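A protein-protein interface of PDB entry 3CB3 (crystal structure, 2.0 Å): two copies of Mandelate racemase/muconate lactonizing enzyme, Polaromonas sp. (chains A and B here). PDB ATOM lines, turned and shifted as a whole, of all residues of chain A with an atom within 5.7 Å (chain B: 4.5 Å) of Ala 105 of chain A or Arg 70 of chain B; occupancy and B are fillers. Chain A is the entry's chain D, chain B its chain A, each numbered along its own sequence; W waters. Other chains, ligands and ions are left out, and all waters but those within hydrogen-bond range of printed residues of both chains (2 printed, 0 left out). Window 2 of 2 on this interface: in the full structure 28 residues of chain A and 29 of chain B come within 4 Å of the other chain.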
ATOM      1  N   GLU A  82      -0.186  21.330 -16.760  1.00  0.00           N
ATOM      2  CA  GLU A  82       0.897  21.884 -15.960  1.00  0.00           C
ATOM      3  C   GLU A  82       1.701  20.845 -15.175  1.00  0.00           C
ATOM      4  O   GLU A  82       2.899  21.034 -14.951  1.00  0.00           O
ATOM      5  CB  GLU A  82       0.336  22.947 -15.012  1.00  0.00           C
ATOM      6  CG  GLU A  82       1.339  23.537 -14.042  1.00  0.00           C
ATOM      7  CD  GLU A  82       0.747  24.677 -13.228  1.00  0.00           C
ATOM      8  OE1 GLU A  82      -0.408  24.538 -12.760  1.00  0.00           O
ATOM      9  OE2 GLU A  82       1.439  25.703 -13.049  1.00  0.00           O
ATOM     10  N   ILE A  83       1.065  19.746 -14.772  1.00  0.00           N
ATOM     11  CA  ILE A  83       1.772  18.716 -14.002  1.00  0.00           C
ATOM     12  C   ILE A  83       2.250  17.506 -14.803  1.00  0.00           C
ATOM     13  O   ILE A  83       3.036  16.701 -14.302  1.00  0.00           O
ATOM     14  CB  ILE A  83       0.907  18.182 -12.832  1.00  0.00           C
ATOM     15  CG1 ILE A  83      -0.308  17.431 -13.383  1.00  0.00           C
ATOM     16  CG2 ILE A  83       0.495  19.344 -11.914  1.00  0.00           C
ATOM     17  CD1 ILE A  83      -1.226  16.883 -12.310  1.00  0.00           C
ATOM     18  N   ALA A  86       6.003  16.174 -14.937  1.00  0.00           N
ATOM     19  CA  ALA A  86       6.572  15.497 -13.773  1.00  0.00           C
ATOM     20  C   ALA A  86       6.599  13.982 -13.935  1.00  0.00           C
ATOM     21  O   ALA A  86       7.265  13.281 -13.169  1.00  0.00           O
ATOM     22  CB  ALA A  86       5.793  15.867 -12.517  1.00  0.00           C
ATOM     23  N   ASP A 100       1.181  10.391  -5.728  1.00  0.00           N
ATOM     24  CA  ASP A 100       1.659  11.290  -4.674  1.00  0.00           C
ATOM     25  C   ASP A 100       2.557  12.388  -5.209  1.00  0.00           C
ATOM     26  O   ASP A 100       2.478  13.535  -4.767  1.00  0.00           O
ATOM     27  CB  ASP A 100       2.430  10.523  -3.603  1.00  0.00           C
ATOM     28  CG  ASP A 100       1.530   9.722  -2.691  1.00  0.00           C
ATOM     29  OD1 ASP A 100       0.338  10.081  -2.562  1.00  0.00           O
ATOM     30  OD2 ASP A 100       2.022   8.743  -2.088  1.00  0.00           O
ATOM     31  N   LYS A 101       3.425  12.041  -6.153  1.00  0.00           N
ATOM     32  CA  LYS A 101       4.326  13.034  -6.716  1.00  0.00           C
ATOM     33  C   LYS A 101       3.552  14.153  -7.402  1.00  0.00           C
ATOM     34  O   LYS A 101       3.835  15.328  -7.185  1.00  0.00           O
ATOM     35  CB  LYS A 101       5.288  12.397  -7.726  1.00  0.00           C
ATOM     36  CG  LYS A 101       6.304  13.396  -8.257  1.00  0.00           C
ATOM     37  CD  LYS A 101       7.211  12.820  -9.330  1.00  0.00           C
ATOM     38  CE  LYS A 101       8.119  13.913  -9.896  1.00  0.00           C
ATOM     39  NZ  LYS A 101       8.909  13.469 -11.083  1.00  0.00           N
ATOM     40  N   LEU A 102       2.575  13.790  -8.229  1.00  0.00           N
ATOM     41  CA  LEU A 102       1.789  14.788  -8.945  1.00  0.00           C
ATOM     42  C   LEU A 102       0.970  15.666  -7.997  1.00  0.00           C
ATOM     43  O   LEU A 102       0.735  16.849  -8.274  1.00  0.00           O
ATOM     44  CB  LEU A 102       0.871  14.113  -9.965  1.00  0.00           C
ATOM     45  CG  LEU A 102       1.567  13.412 -11.136  1.00  0.00           C
ATOM     46  CD1 LEU A 102       0.551  13.138 -12.221  1.00  0.00           C
ATOM     47  CD2 LEU A 102       2.687  14.288 -11.694  1.00  0.00           C
ATOM     48  N   CYS A 103       0.543  15.076  -6.885  1.00  0.00           N
ATOM     49  CA  CYS A 103      -0.227  15.787  -5.870  1.00  0.00           C
ATOM     50  C   CYS A 103       0.686  16.871  -5.292  1.00  0.00           C
ATOM     51  O   CYS A 103       0.286  18.027  -5.144  1.00  0.00           O
ATOM     52  CB  CYS A 103      -0.653  14.806  -4.776  1.00  0.00           C
ATOM     53  SG  CYS A 103      -2.175  15.238  -3.909  1.00  0.00           S
ATOM     54  N   TRP A 104       1.923  16.490  -4.979  1.00  0.00           N
ATOM     55  CA  TRP A 104       2.899  17.433  -4.447  1.00  0.00           C
ATOM     56  C   TRP A 104       3.211  18.520  -5.462  1.00  0.00           C
ATOM     57  O   TRP A 104       3.442  19.665  -5.089  1.00  0.00           O
ATOM     58  CB  TRP A 104       4.195  16.717  -4.059  1.00  0.00           C
ATOM     59  CG  TRP A 104       4.108  16.022  -2.749  1.00  0.00           C
ATOM     60  CD1 TRP A 104       4.169  14.678  -2.528  1.00  0.00           C
ATOM     61  CD2 TRP A 104       3.911  16.633  -1.468  1.00  0.00           C
ATOM     62  NE1 TRP A 104       4.019  14.411  -1.189  1.00  0.00           N
ATOM     63  CE2 TRP A 104       3.859  15.593  -0.513  1.00  0.00           C
ATOM     64  CE3 TRP A 104       3.773  17.960  -1.032  1.00  0.00           C
ATOM     65  CZ2 TRP A 104       3.672  15.837   0.856  1.00  0.00           C
ATOM     66  CZ3 TRP A 104       3.587  18.204   0.329  1.00  0.00           C
ATOM     67  CH2 TRP A 104       3.539  17.144   1.256  1.00  0.00           C
ATOM     68  N   ALA A 105       3.217  18.166  -6.745  1.00  0.00           N
ATOM     69  CA  ALA A 105       3.490  19.147  -7.793  1.00  0.00           C
ATOM     70  C   ALA A 105       2.498  20.297  -7.666  1.00  0.00           C
ATOM     71  O   ALA A 105       2.777  21.420  -8.089  1.00  0.00           O
ATOM     72  CB  ALA A 105       3.371  18.505  -9.175  1.00  0.00           C
ATOM     73  N   GLY A 106       1.331  19.999  -7.095  1.00  0.00           N
ATOM     74  CA  GLY A 106       0.306  21.010  -6.888  1.00  0.00           C
ATOM     75  C   GLY A 106      -0.110  20.949  -5.430  1.00  0.00           C
ATOM     76  O   GLY A 106      -1.293  20.834  -5.104  1.00  0.00           O
ATOM     77  N   ALA A 107       0.884  21.030  -4.553  1.00  0.00           N
ATOM     78  CA  ALA A 107       0.680  20.952  -3.109  1.00  0.00           C
ATOM     79  C   ALA A 107      -0.402  21.860  -2.508  1.00  0.00           C
ATOM     80  O   ALA A 107      -1.146  21.431  -1.624  1.00  0.00           O
ATOM     81  CB  ALA A 107       2.007  21.192  -2.403  1.00  0.00           C
ATOM     82  N   SER A 108      -0.492  23.103  -2.973  1.00  0.00           N
ATOM     83  CA  SER A 108      -1.492  24.023  -2.427  1.00  0.00           C
ATOM     84  C   SER A 108      -2.854  23.812  -3.067  1.00  0.00           C
ATOM     85  O   SER A 108      -3.829  24.454  -2.688  1.00  0.00           O
ATOM     86  CB  SER A 108      -1.062  25.478  -2.640  1.00  0.00           C
ATOM     87  OG  SER A 108      -1.173  25.852  -4.005  1.00  0.00           O
ATOM     88  N   ASP B  33      13.146  24.269  -0.595  1.00  0.00           N
ATOM     89  CA  ASP B  33      13.012  23.441   0.596  1.00  0.00           C
ATOM     90  C   ASP B  33      13.896  22.204   0.468  1.00  0.00           C
ATOM     91  O   ASP B  33      14.758  22.132  -0.410  1.00  0.00           O
ATOM     92  CB  ASP B  33      11.555  23.012   0.775  1.00  0.00           C
ATOM     93  CG  ASP B  33      11.065  22.141  -0.364  1.00  0.00           C
ATOM     94  OD1 ASP B  33      11.099  22.599  -1.527  1.00  0.00           O
ATOM     95  OD2 ASP B  33      10.649  20.993  -0.098  1.00  0.00           O
ATOM     96  N   VAL B  36      13.866  20.402  -2.871  1.00  0.00           N
ATOM     97  CA  VAL B  36      14.676  21.032  -3.904  1.00  0.00           C
ATOM     98  C   VAL B  36      16.135  20.633  -3.714  1.00  0.00           C
ATOM     99  O   VAL B  36      16.794  20.204  -4.656  1.00  0.00           O
ATOM    100  CB  VAL B  36      14.558  22.579  -3.851  1.00  0.00           C
ATOM    101  CG1 VAL B  36      15.525  23.215  -4.841  1.00  0.00           C
ATOM    102  CG2 VAL B  36      13.125  23.004  -4.166  1.00  0.00           C
ATOM    103  N   GLN B  41      12.743  18.480  -7.053  1.00  0.00           N
ATOM    104  CA  GLN B  41      11.841  19.537  -7.481  1.00  0.00           C
ATOM    105  C   GLN B  41      12.601  20.841  -7.698  1.00  0.00           C
ATOM    106  O   GLN B  41      13.635  21.078  -7.075  1.00  0.00           O
ATOM    107  CB  GLN B  41      10.756  19.711  -6.410  1.00  0.00           C
ATOM    108  CG  GLN B  41       9.680  20.722  -6.706  1.00  0.00           C
ATOM    109  CD  GLN B  41       8.556  20.654  -5.683  1.00  0.00           C
ATOM    110  OE1 GLN B  41       8.798  20.669  -4.473  1.00  0.00           O
ATOM    111  NE2 GLN B  41       7.321  20.576  -6.167  1.00  0.00           N
ATOM    112  N   LYS B  42      12.087  21.670  -8.600  1.00  0.00           N
ATOM    113  CA  LYS B  42      12.694  22.958  -8.913  1.00  0.00           C
ATOM    114  C   LYS B  42      12.371  23.997  -7.849  1.00  0.00           C
ATOM    115  O   LYS B  42      11.360  23.902  -7.154  1.00  0.00           O
ATOM    116  CB  LYS B  42      12.187  23.470 -10.262  1.00  0.00           C
ATOM    117  CG  LYS B  42      12.693  22.700 -11.467  1.00  0.00           C
ATOM    118  CD  LYS B  42      12.115  23.267 -12.757  1.00  0.00           C
ATOM    119  CE  LYS B  42      12.995  22.921 -13.959  1.00  0.00           C
ATOM    120  NZ  LYS B  42      13.237  21.459 -14.093  1.00  0.00           N
ATOM    121  N   PRO B  43      13.243  25.000  -7.697  1.00  0.00           N
ATOM    122  CA  PRO B  43      12.988  26.039  -6.695  1.00  0.00           C
ATOM    123  C   PRO B  43      11.741  26.815  -7.126  1.00  0.00           C
ATOM    124  O   PRO B  43      11.412  26.858  -8.316  1.00  0.00           O
ATOM    125  CB  PRO B  43      14.241  26.915  -6.772  1.00  0.00           C
ATOM    126  CG  PRO B  43      15.304  25.967  -7.252  1.00  0.00           C
ATOM    127  CD  PRO B  43      14.578  25.160  -8.301  1.00  0.00           C
ATOM    128  N   MET B  44      11.051  27.411  -6.160  1.00  0.00           N
ATOM    129  CA  MET B  44       9.863  28.208  -6.441  1.00  0.00           C
ATOM    130  C   MET B  44      10.373  29.619  -6.722  1.00  0.00           C
ATOM    131  O   MET B  44      11.019  30.217  -5.864  1.00  0.00           O
ATOM    132  CB  MET B  44       8.947  28.218  -5.218  1.00  0.00           C
ATOM    133  CG  MET B  44       7.564  28.804  -5.455  1.00  0.00           C
ATOM    134  SD  MET B  44       6.637  28.938  -3.905  1.00  0.00           S
ATOM    135  CE  MET B  44       6.962  27.309  -3.181  1.00  0.00           C
ATOM    136  N   SER B  68      -1.714  30.347  -6.076  1.00  0.00           N
ATOM    137  CA  SER B  68      -1.211  28.979  -6.079  1.00  0.00           C
ATOM    138  C   SER B  68       0.304  29.087  -5.979  1.00  0.00           C
ATOM    139  O   SER B  68       0.925  29.794  -6.766  1.00  0.00           O
ATOM    140  CB  SER B  68      -1.577  28.260  -7.381  1.00  0.00           C
ATOM    141  OG  SER B  68      -2.977  28.131  -7.539  1.00  0.00           O
ATOM    142  N   LYS B  69       0.895  28.396  -5.013  1.00  0.00           N
ATOM    143  CA  LYS B  69       2.345  28.433  -4.835  1.00  0.00           C
ATOM    144  C   LYS B  69       3.042  27.565  -5.876  1.00  0.00           C
ATOM    145  O   LYS B  69       3.957  28.021  -6.567  1.00  0.00           O
ATOM    146  CB  LYS B  69       2.711  27.998  -3.411  1.00  0.00           C
ATOM    147  CG  LYS B  69       2.024  26.733  -2.917  1.00  0.00           C
ATOM    148  CD  LYS B  69       2.932  25.511  -3.005  1.00  0.00           C
ATOM    149  CE  LYS B  69       4.260  25.739  -2.279  1.00  0.00           C
ATOM    150  NZ  LYS B  69       4.088  26.201  -0.871  1.00  0.00           N
ATOM    151  N   ARG B  70       2.616  26.314  -5.996  1.00  0.00           N
ATOM    152  CA  ARG B  70       3.195  25.426  -7.001  1.00  0.00           C
ATOM    153  C   ARG B  70       2.179  25.350  -8.139  1.00  0.00           C
ATOM    154  O   ARG B  70       1.554  26.356  -8.465  1.00  0.00           O
ATOM    155  CB  ARG B  70       3.457  24.040  -6.406  1.00  0.00           C
ATOM    156  CG  ARG B  70       4.625  23.995  -5.426  1.00  0.00           C
ATOM    157  CD  ARG B  70       5.958  24.147  -6.140  1.00  0.00           C
ATOM    158  NE  ARG B  70       7.107  24.021  -5.238  1.00  0.00           N
ATOM    159  CZ  ARG B  70       8.375  23.993  -5.650  1.00  0.00           C
ATOM    160  NH1 ARG B  70       8.656  24.075  -6.946  1.00  0.00           N
ATOM    161  NH2 ARG B  70       9.369  23.893  -4.773  1.00  0.00           N
ATOM    162  N   ALA B  71       1.999  24.177  -8.738  1.00  0.00           N
ATOM    163  CA  ALA B  71       1.039  24.045  -9.832  1.00  0.00           C
ATOM    164  C   ALA B  71      -0.372  24.361  -9.333  1.00  0.00           C
ATOM    165  O   ALA B  71      -0.696  24.091  -8.180  1.00  0.00           O
ATOM    166  CB  ALA B  71       1.081  22.624 -10.406  1.00  0.00           C
ATOM    167  N   GLY B  72      -1.202  24.934 -10.198  1.00  0.00           N
ATOM    168  CA  GLY B  72      -2.565  25.252  -9.803  1.00  0.00           C
ATOM    169  C   GLY B  72      -3.113  26.560 -10.354  1.00  0.00           C
ATOM    170  O   GLY B  72      -4.331  26.738 -10.434  1.00  0.00           O
HETATM  171  O   HOH W   1       0.658  27.734 -11.040  1.00  0.00           O
HETATM  172  O   HOH W   2      -3.055  24.411 -12.746  1.00  0.00           O
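Ala 71 of chain B touches Glu 82 of chain A.
CG2 of Ile 83 of chain A touches CB of Ala 71 of chain B, at 3.7 Å.
O of Ala 105 of chain A touches CB of Arg 70 of chain B (3.2 Å).
Ala 71 of chain B touches Gly 106 of chain A (O to CA, 3.5 Å).
Ser 108 of chain A touches Ser 68 of chain B.
The backbone NH (N) of Lys 69 of chain B lies within hydrogen-bond range of the side-chain hydroxyl (OG) of Ser 108 of chain A (3.4 Å).
The backbone carbonyl oxygen (O) of Ala 105 of chain A is in hydrogen-bond range of the backbone NH (N) of Ala 71 of chain B (2.9 Å).
The side-chain carboxylate (OE1) of Glu 82 of chain A is in hydrogen-bond range of the backbone NH (N) of Gly 72 of chain B (2.7 Å).
Water W2 lies within hydrogen-bond range of the side-chain carboxylate (OE1) of Glu 82 of chain A (2.7 Å) and the backbone NH (N) of Gly 72 of chain B (3.2 Å).
Water W1 lies within hydrogen-bond range of the side-chain carboxylate (OE2) of Glu 82 of chain A (3.0 Å), the backbone carbonyl oxygen (O) of Arg 70 of chain B (3.1 Å) and the backbone NH (N) of Gly 72 of chain B (3.5 Å).
No position is printed for both chains.
Of the 8 pairs that touch across the chains among the printed residues, none has its exchanged pair printed and touching as well.
Ala 105 of chain A touches just these residues of chain B: Arg 70 (3.2 Å) and Ala 71 (2.9 Å).
Of the printed residues of chain A, Arg 70 of chain B touches Ala 105.
Of the printed residues of chain A, Lys 69 of chain B touches Ser 108.
Printed residues of chain B within 4 Å of Ser 108 of chain A: Ser 68 and Lys 69.
Of the printed residues of chain A, Gly 72 of chain B touches Glu 82.
Of the printed residues of chain A, Ala 71 of chain B touches Glu 82 (3.3 Å), Ile 83 (3.7 Å), Ala 105 (2.9 Å) and Gly 106 (3.5 Å).
Ala 107 of chain A touches none of the printed residues of chain B.
The nearest printed residue of chain A that does not touch Ser 68 of chain B is Glu 82 of chain A (6.6 Å).
OD1 of Asp 33 of chain B lies within salt-bridge range of NH2 of Arg 70 of chain B.
The side-chain amide oxygen of Gln 41 of chain B lies within hydrogen-bond range of the guanidinium group of Arg 70 of chain B.
The backbone carbonyl oxygen (O) of Lys 42 of chain B is in hydrogen-bond range of the guanidinium group (NH1) of Arg 70 of chain B.
OG of Ser 68 of chain B lies close to O of Gly 72 of chain B, 3.5 Å away.
Along chain B the printed residues that touch a printed residue of chain A span positions 68 to 72.
Hydrophobic or aromatic side chains of chain A that line the printed part of chain B: Ile 83.
Along chain A the printed residues that touch a printed residue of chain B span positions 82 to 108.
Among the printed residues, no Asp or Glu carboxylate lies within 4 Å of a Lys or Arg side-chain nitrogen of the other chain.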
